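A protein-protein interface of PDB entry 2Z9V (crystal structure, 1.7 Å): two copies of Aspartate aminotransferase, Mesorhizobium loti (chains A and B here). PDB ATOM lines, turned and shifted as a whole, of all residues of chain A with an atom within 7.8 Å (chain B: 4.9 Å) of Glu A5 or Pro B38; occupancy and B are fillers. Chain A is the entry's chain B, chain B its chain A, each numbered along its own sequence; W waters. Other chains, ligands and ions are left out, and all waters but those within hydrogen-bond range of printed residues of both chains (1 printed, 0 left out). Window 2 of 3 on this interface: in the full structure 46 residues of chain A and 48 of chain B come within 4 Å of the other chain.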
ATOM      1  N   ARG A   2       5.081 -14.930 -19.106  1.00  0.00           N
ATOM      2  CA  ARG A   2       6.452 -15.003 -18.611  1.00  0.00           C
ATOM      3  C   ARG A   2       6.504 -14.559 -17.159  1.00  0.00           C
ATOM      4  O   ARG A   2       5.822 -13.608 -16.766  1.00  0.00           O
ATOM      5  CB  ARG A   2       7.390 -14.131 -19.460  1.00  0.00           C
ATOM      6  CG  ARG A   2       7.672 -14.633 -20.892  1.00  0.00           C
ATOM      7  CD  ARG A   2       8.125 -16.094 -20.919  1.00  0.00           C
ATOM      8  NE  ARG A   2       8.148 -16.621 -22.278  1.00  0.00           N
ATOM      9  CZ  ARG A   2       9.255 -16.798 -22.986  1.00  0.00           C
ATOM     10  NH1 ARG A   2       9.177 -17.285 -24.220  1.00  0.00           N
ATOM     11  NH2 ARG A   2      10.439 -16.501 -22.456  1.00  0.00           N
ATOM     12  N   TYR A   3       7.317 -15.249 -16.360  1.00  0.00           N
ATOM     13  CA  TYR A   3       7.537 -14.869 -14.975  1.00  0.00           C
ATOM     14  C   TYR A   3       8.680 -13.874 -14.884  1.00  0.00           C
ATOM     15  O   TYR A   3       9.799 -14.166 -15.315  1.00  0.00           O
ATOM     16  CB  TYR A   3       7.833 -16.103 -14.117  1.00  0.00           C
ATOM     17  CG  TYR A   3       6.638 -17.011 -14.003  1.00  0.00           C
ATOM     18  CD1 TYR A   3       6.423 -18.033 -14.928  1.00  0.00           C
ATOM     19  CD2 TYR A   3       5.692 -16.826 -12.986  1.00  0.00           C
ATOM     20  CE1 TYR A   3       5.308 -18.858 -14.837  1.00  0.00           C
ATOM     21  CE2 TYR A   3       4.567 -17.636 -12.892  1.00  0.00           C
ATOM     22  CZ  TYR A   3       4.383 -18.658 -13.812  1.00  0.00           C
ATOM     23  OH  TYR A   3       3.275 -19.474 -13.708  1.00  0.00           O
ATOM     24  N   PRO A   4       8.402 -12.678 -14.345  1.00  0.00           N
ATOM     25  CA  PRO A   4       9.502 -11.717 -14.263  1.00  0.00           C
ATOM     26  C   PRO A   4      10.568 -12.128 -13.245  1.00  0.00           C
ATOM     27  O   PRO A   4      10.264 -12.770 -12.231  1.00  0.00           O
ATOM     28  CB  PRO A   4       8.822 -10.410 -13.823  1.00  0.00           C
ATOM     29  CG  PRO A   4       7.332 -10.652 -13.904  1.00  0.00           C
ATOM     30  CD  PRO A   4       7.132 -12.144 -13.814  1.00  0.00           C
ATOM     31  N   GLU A   5      11.812 -11.752 -13.527  1.00  0.00           N
ATOM     32  CA  GLU A   5      12.935 -12.067 -12.643  1.00  0.00           C
ATOM     33  C   GLU A   5      12.784 -11.463 -11.250  1.00  0.00           C
ATOM     34  O   GLU A   5      13.195 -12.074 -10.255  1.00  0.00           O
ATOM     35  CB  GLU A   5      14.248 -11.616 -13.286  1.00  0.00           C
ATOM     36  CG  GLU A   5      14.600 -12.409 -14.524  1.00  0.00           C
ATOM     37  CD  GLU A   5      15.956 -12.057 -15.081  1.00  0.00           C
ATOM     38  OE1 GLU A   5      16.669 -11.244 -14.454  1.00  0.00           O
ATOM     39  OE2 GLU A   5      16.306 -12.595 -16.151  1.00  0.00           O
ATOM     40  N   HIS A   6      12.182 -10.272 -11.184  1.00  0.00           N
ATOM     41  CA  HIS A   6      12.004  -9.555  -9.918  1.00  0.00           C
ATOM     42  C   HIS A   6      10.888 -10.146  -9.065  1.00  0.00           C
ATOM     43  O   HIS A   6      10.881  -9.980  -7.848  1.00  0.00           O
ATOM     44  CB  HIS A   6      11.767  -8.054 -10.164  1.00  0.00           C
ATOM     45  CG  HIS A   6      10.468  -7.741 -10.855  1.00  0.00           C
ATOM     46  ND1 HIS A   6      10.391  -7.462 -12.204  1.00  0.00           N
ATOM     47  CD2 HIS A   6       9.201  -7.656 -10.382  1.00  0.00           C
ATOM     48  CE1 HIS A   6       9.135  -7.219 -12.530  1.00  0.00           C
ATOM     49  NE2 HIS A   6       8.392  -7.338 -11.445  1.00  0.00           N
ATOM     50  N   ALA A   7       9.953 -10.848  -9.704  1.00  0.00           N
ATOM     51  CA  ALA A   7       8.833 -11.469  -8.998  1.00  0.00           C
ATOM     52  C   ALA A   7       9.246 -12.841  -8.470  1.00  0.00           C
ATOM     53  O   ALA A   7      10.143 -13.474  -9.029  1.00  0.00           O
ATOM     54  CB  ALA A   7       7.627 -11.584  -9.910  1.00  0.00           C
ATOM     55  N   ASP A   8       8.603 -13.271  -7.386  1.00  0.00           N
ATOM     56  CA  ASP A   8       8.833 -14.599  -6.800  1.00  0.00           C
ATOM     57  C   ASP A   8       8.492 -15.730  -7.782  1.00  0.00           C
ATOM     58  O   ASP A   8       7.607 -15.583  -8.625  1.00  0.00           O
ATOM     59  CB  ASP A   8       8.022 -14.758  -5.503  1.00  0.00           C
ATOM     60  CG  ASP A   8       8.756 -14.233  -4.268  1.00  0.00           C
ATOM     61  OD1 ASP A   8       9.720 -13.448  -4.403  1.00  0.00           O
ATOM     62  OD2 ASP A   8       8.368 -14.613  -3.136  1.00  0.00           O
ATOM     63  N   PRO A   9       9.196 -16.874  -7.676  1.00  0.00           N
ATOM     64  CA  PRO A   9       8.859 -17.991  -8.557  1.00  0.00           C
ATOM     65  C   PRO A   9       7.662 -18.784  -8.012  1.00  0.00           C
ATOM     66  O   PRO A   9       7.163 -18.490  -6.911  1.00  0.00           O
ATOM     67  CB  PRO A   9      10.121 -18.841  -8.503  1.00  0.00           C
ATOM     68  CG  PRO A   9      10.551 -18.703  -7.047  1.00  0.00           C
ATOM     69  CD  PRO A   9      10.302 -17.218  -6.757  1.00  0.00           C
ATOM     70  N   ARG A 320      18.115 -22.717 -17.484  1.00  0.00           N
ATOM     71  CA  ARG A 320      17.547 -22.427 -16.161  1.00  0.00           C
ATOM     72  C   ARG A 320      16.727 -21.152 -16.192  1.00  0.00           C
ATOM     73  O   ARG A 320      15.663 -21.071 -15.577  1.00  0.00           O
ATOM     74  CB  ARG A 320      18.638 -22.310 -15.091  1.00  0.00           C
ATOM     75  CG  ARG A 320      19.208 -23.639 -14.643  1.00  0.00           C
ATOM     76  CD  ARG A 320      20.260 -23.446 -13.545  1.00  0.00           C
ATOM     77  NE  ARG A 320      21.505 -22.889 -14.072  1.00  0.00           N
ATOM     78  CZ  ARG A 320      21.872 -21.616 -13.932  1.00  0.00           C
ATOM     79  NH1 ARG A 320      21.110 -20.774 -13.237  1.00  0.00           N
ATOM     80  NH2 ARG A 320      23.026 -21.194 -14.440  1.00  0.00           N
ATOM     81  N   GLN A 321      17.225 -20.157 -16.909  1.00  0.00           N
ATOM     82  CA  GLN A 321      16.490 -18.911 -17.065  1.00  0.00           C
ATOM     83  C   GLN A 321      15.154 -19.155 -17.740  1.00  0.00           C
ATOM     84  O   GLN A 321      14.137 -18.600 -17.313  1.00  0.00           O
ATOM     85  CB  GLN A 321      17.324 -17.896 -17.842  1.00  0.00           C
ATOM     86  CG  GLN A 321      18.473 -17.329 -17.022  1.00  0.00           C
ATOM     87  CD  GLN A 321      19.343 -16.382 -17.821  1.00  0.00           C
ATOM     88  OE1 GLN A 321      20.013 -15.504 -17.258  1.00  0.00           O
ATOM     89  NE2 GLN A 321      19.347 -16.554 -19.141  1.00  0.00           N
ATOM     90  N   ARG A 324      12.563 -20.960 -15.394  1.00  0.00           N
ATOM     91  CA  ARG A 324      11.944 -20.016 -14.466  1.00  0.00           C
ATOM     92  C   ARG A 324      10.999 -19.061 -15.189  1.00  0.00           C
ATOM     93  O   ARG A 324       9.885 -18.843 -14.734  1.00  0.00           O
ATOM     94  CB  ARG A 324      12.995 -19.249 -13.661  1.00  0.00           C
ATOM     95  CG  ARG A 324      12.408 -18.521 -12.439  1.00  0.00           C
ATOM     96  CD  ARG A 324      13.480 -17.623 -11.823  1.00  0.00           C
ATOM     97  NE  ARG A 324      13.104 -17.022 -10.537  1.00  0.00           N
ATOM     98  CZ  ARG A 324      12.298 -15.963 -10.396  1.00  0.00           C
ATOM     99  NH1 ARG A 324      11.705 -15.401 -11.453  1.00  0.00           N
ATOM    100  NH2 ARG A 324      12.066 -15.470  -9.183  1.00  0.00           N
ATOM    101  N   ALA A 325      11.430 -18.511 -16.328  1.00  0.00           N
ATOM    102  CA  ALA A 325      10.620 -17.545 -17.058  1.00  0.00           C
ATOM    103  C   ALA A 325       9.355 -18.147 -17.680  1.00  0.00           C
ATOM    104  O   ALA A 325       8.308 -17.509 -17.689  1.00  0.00           O
ATOM    105  CB  ALA A 325      11.450 -16.830 -18.115  1.00  0.00           C
ATOM    106  N   VAL A 330      12.365 -23.114 -10.424  1.00  0.00           N
ATOM    107  CA  VAL A 330      13.771 -22.751 -10.229  1.00  0.00           C
ATOM    108  C   VAL A 330      14.619 -23.996  -9.984  1.00  0.00           C
ATOM    109  O   VAL A 330      14.309 -24.819  -9.103  1.00  0.00           O
ATOM    110  CB  VAL A 330      13.948 -21.748  -9.069  1.00  0.00           C
ATOM    111  CG1 VAL A 330      15.401 -21.243  -8.992  1.00  0.00           C
ATOM    112  CG2 VAL A 330      12.957 -20.597  -9.225  1.00  0.00           C
ATOM    113  N   TYR B  36      20.640 -17.885  -5.376  1.00  0.00           N
ATOM    114  CA  TYR B  36      20.932 -17.468  -6.753  1.00  0.00           C
ATOM    115  C   TYR B  36      19.685 -17.233  -7.615  1.00  0.00           C
ATOM    116  O   TYR B  36      19.781 -17.018  -8.832  1.00  0.00           O
ATOM    117  CB  TYR B  36      21.944 -18.425  -7.403  1.00  0.00           C
ATOM    118  CG  TYR B  36      23.311 -18.267  -6.769  1.00  0.00           C
ATOM    119  CD1 TYR B  36      23.662 -18.998  -5.637  1.00  0.00           C
ATOM    120  CD2 TYR B  36      24.227 -17.325  -7.265  1.00  0.00           C
ATOM    121  CE1 TYR B  36      24.900 -18.827  -5.020  1.00  0.00           C
ATOM    122  CE2 TYR B  36      25.471 -17.141  -6.659  1.00  0.00           C
ATOM    123  CZ  TYR B  36      25.796 -17.895  -5.530  1.00  0.00           C
ATOM    124  OH  TYR B  36      27.021 -17.734  -4.914  1.00  0.00           O
ATOM    125  N   ASP B  37      18.518 -17.250  -6.984  1.00  0.00           N
ATOM    126  CA  ASP B  37      17.298 -16.831  -7.655  1.00  0.00           C
ATOM    127  C   ASP B  37      17.415 -15.327  -7.908  1.00  0.00           C
ATOM    128  O   ASP B  37      17.868 -14.586  -7.025  1.00  0.00           O
ATOM    129  CB  ASP B  37      16.082 -17.128  -6.773  1.00  0.00           C
ATOM    130  CG  ASP B  37      14.763 -16.825  -7.468  1.00  0.00           C
ATOM    131  OD1 ASP B  37      14.430 -15.637  -7.632  1.00  0.00           O
ATOM    132  OD2 ASP B  37      14.028 -17.771  -7.809  1.00  0.00           O
ATOM    133  N   PRO B  38      17.036 -14.874  -9.116  1.00  0.00           N
ATOM    134  CA  PRO B  38      17.163 -13.444  -9.387  1.00  0.00           C
ATOM    135  C   PRO B  38      16.381 -12.544  -8.418  1.00  0.00           C
ATOM    136  O   PRO B  38      16.827 -11.419  -8.141  1.00  0.00           O
ATOM    137  CB  PRO B  38      16.630 -13.309 -10.825  1.00  0.00           C
ATOM    138  CG  PRO B  38      15.737 -14.517 -11.016  1.00  0.00           C
ATOM    139  CD  PRO B  38      16.504 -15.604 -10.284  1.00  0.00           C
ATOM    140  N   ALA B  39      15.251 -13.028  -7.896  1.00  0.00           N
ATOM    141  CA  ALA B  39      14.450 -12.243  -6.956  1.00  0.00           C
ATOM    142  C   ALA B  39      15.189 -12.081  -5.625  1.00  0.00           C
ATOM    143  O   ALA B  39      15.099 -11.030  -4.985  1.00  0.00           O
ATOM    144  CB  ALA B  39      13.097 -12.881  -6.738  1.00  0.00           C
ATOM    145  N   PHE B  40      15.928 -13.110  -5.221  1.00  0.00           N
ATOM    146  CA  PHE B  40      16.741 -12.973  -4.019  1.00  0.00           C
ATOM    147  C   PHE B  40      17.960 -12.071  -4.228  1.00  0.00           C
ATOM    148  O   PHE B  40      18.310 -11.273  -3.353  1.00  0.00           O
ATOM    149  CB  PHE B  40      17.179 -14.308  -3.426  1.00  0.00           C
ATOM    150  CG  PHE B  40      17.915 -14.134  -2.131  1.00  0.00           C
ATOM    151  CD1 PHE B  40      19.313 -14.113  -2.104  1.00  0.00           C
ATOM    152  CD2 PHE B  40      17.205 -13.910  -0.944  1.00  0.00           C
ATOM    153  CE1 PHE B  40      19.998 -13.905  -0.901  1.00  0.00           C
ATOM    154  CE2 PHE B  40      17.882 -13.699   0.265  1.00  0.00           C
ATOM    155  CZ  PHE B  40      19.281 -13.704   0.279  1.00  0.00           C
ATOM    156  N   GLN B  41      18.595 -12.187  -5.393  1.00  0.00           N
ATOM    157  CA  GLN B  41      19.759 -11.364  -5.702  1.00  0.00           C
ATOM    158  C   GLN B  41      19.351  -9.890  -5.661  1.00  0.00           C
ATOM    159  O   GLN B  41      20.102  -9.043  -5.151  1.00  0.00           O
ATOM    160  CB  GLN B  41      20.312 -11.737  -7.074  1.00  0.00           C
ATOM    161  CG  GLN B  41      20.971 -13.126  -7.091  1.00  0.00           C
ATOM    162  CD  GLN B  41      22.414 -13.074  -6.662  1.00  0.00           C
ATOM    163  OE1 GLN B  41      22.781 -12.291  -5.783  1.00  0.00           O
ATOM    164  NE2 GLN B  41      23.254 -13.916  -7.281  1.00  0.00           N
ATOM    165  N   LEU B  42      18.166  -9.591  -6.193  1.00  0.00           N
ATOM    166  CA  LEU B  42      17.641  -8.225  -6.140  1.00  0.00           C
ATOM    167  C   LEU B  42      17.351  -7.816  -4.695  1.00  0.00           C
ATOM    168  O   LEU B  42      17.765  -6.733  -4.272  1.00  0.00           O
ATOM    169  CB  LEU B  42      16.387  -8.087  -7.006  1.00  0.00           C
ATOM    170  CG  LEU B  42      15.743  -6.704  -7.123  1.00  0.00           C
ATOM    171  CD1 LEU B  42      16.762  -5.680  -7.598  1.00  0.00           C
ATOM    172  CD2 LEU B  42      14.537  -6.773  -8.065  1.00  0.00           C
HETATM  173  O   HOH W   1      20.472 -19.046 -10.653  1.00  0.00           O
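Of the printed residues of chain B, Glu A5 touches Pro B38 (3.6 Å) and Ala B39 (3.3 Å).
Of chain A, only Glu A5 and Arg A324 come within 4 Å of Pro B38.
Of chain A, only Glu A5 (3.3 Å), His A6 (3.8 Å), Ala A7 (3.8 Å) and Arg A324 (3.7 Å) come within 4 Å of Ala B39.
Of the printed residues of chain B, Pro A9 touches Asp B37.
Of the printed residues of chain B, Val A330 touches Asp B37 (3.3 Å).
Of the printed residues of chain B, Arg A324 touches Asp B37 (2.8 Å), Pro B38 (3.7 Å) and Ala B39 (3.7 Å).
Asp A8 touches none of the printed residues of chain B.
Phe B40 touches none of the printed residues of chain A.
No position is printed for both chains.
Of the 10 pairs that touch across the chains among the printed residues, none has its exchanged pair printed and touching as well.
The side-chain carboxylate (OD1) of Asp B37 is in hydrogen-bond range of the backbone NH (N) of Ala B39 (2.7 Å).
O of Pro A4 is in hydrogen-bond range of NH1 of Arg A324 (3.1 Å).
NH2 of Arg A324 lies within hydrogen-bond range of O of Ala A7, 2.8 Å away.
Water W1 bridges O of Tyr B36 and NH1 of Arg A320.
Of the 7 printed residues of chain B, 4 touch a printed residue of chain A.
Hydrophobic or aromatic side chains of chain B within 4 Å of the printed part of chain A: Pro B38, Ala B39 and Leu B42.
Along chain B the printed residues that touch a printed residue of chain A span positions 37 to 42.
Among the printed residues, Asp or Glu carboxylates within 4 Å of a Lys or Arg side-chain nitrogen of the other chain: Arg A324 with Asp B37.
OD1 of Asp B37 lies within salt-bridge range of NH2 of Arg A324.
The backbone NH (N) of Ala B39 sits at hydrogen-bond distance from the backbone carbonyl oxygen (O) of Glu A5 (3.3 Å).
Among the printed residues, pairs that only touch across the chains: Val A330 with Asp B37 (3.3 Å), Glu A5 with Pro B38 (3.6 Å), Arg A324 with Pro B38 (3.7 Å), Pro A9 with Asp B37 (3.7 Å), His A6 with Leu B42 (3.7 Å), Arg A324 with Ala B39 (3.7 Å), Ala A7 with Ala B39 (3.8 Å) and His A6 with Ala B39 (3.8 Å).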
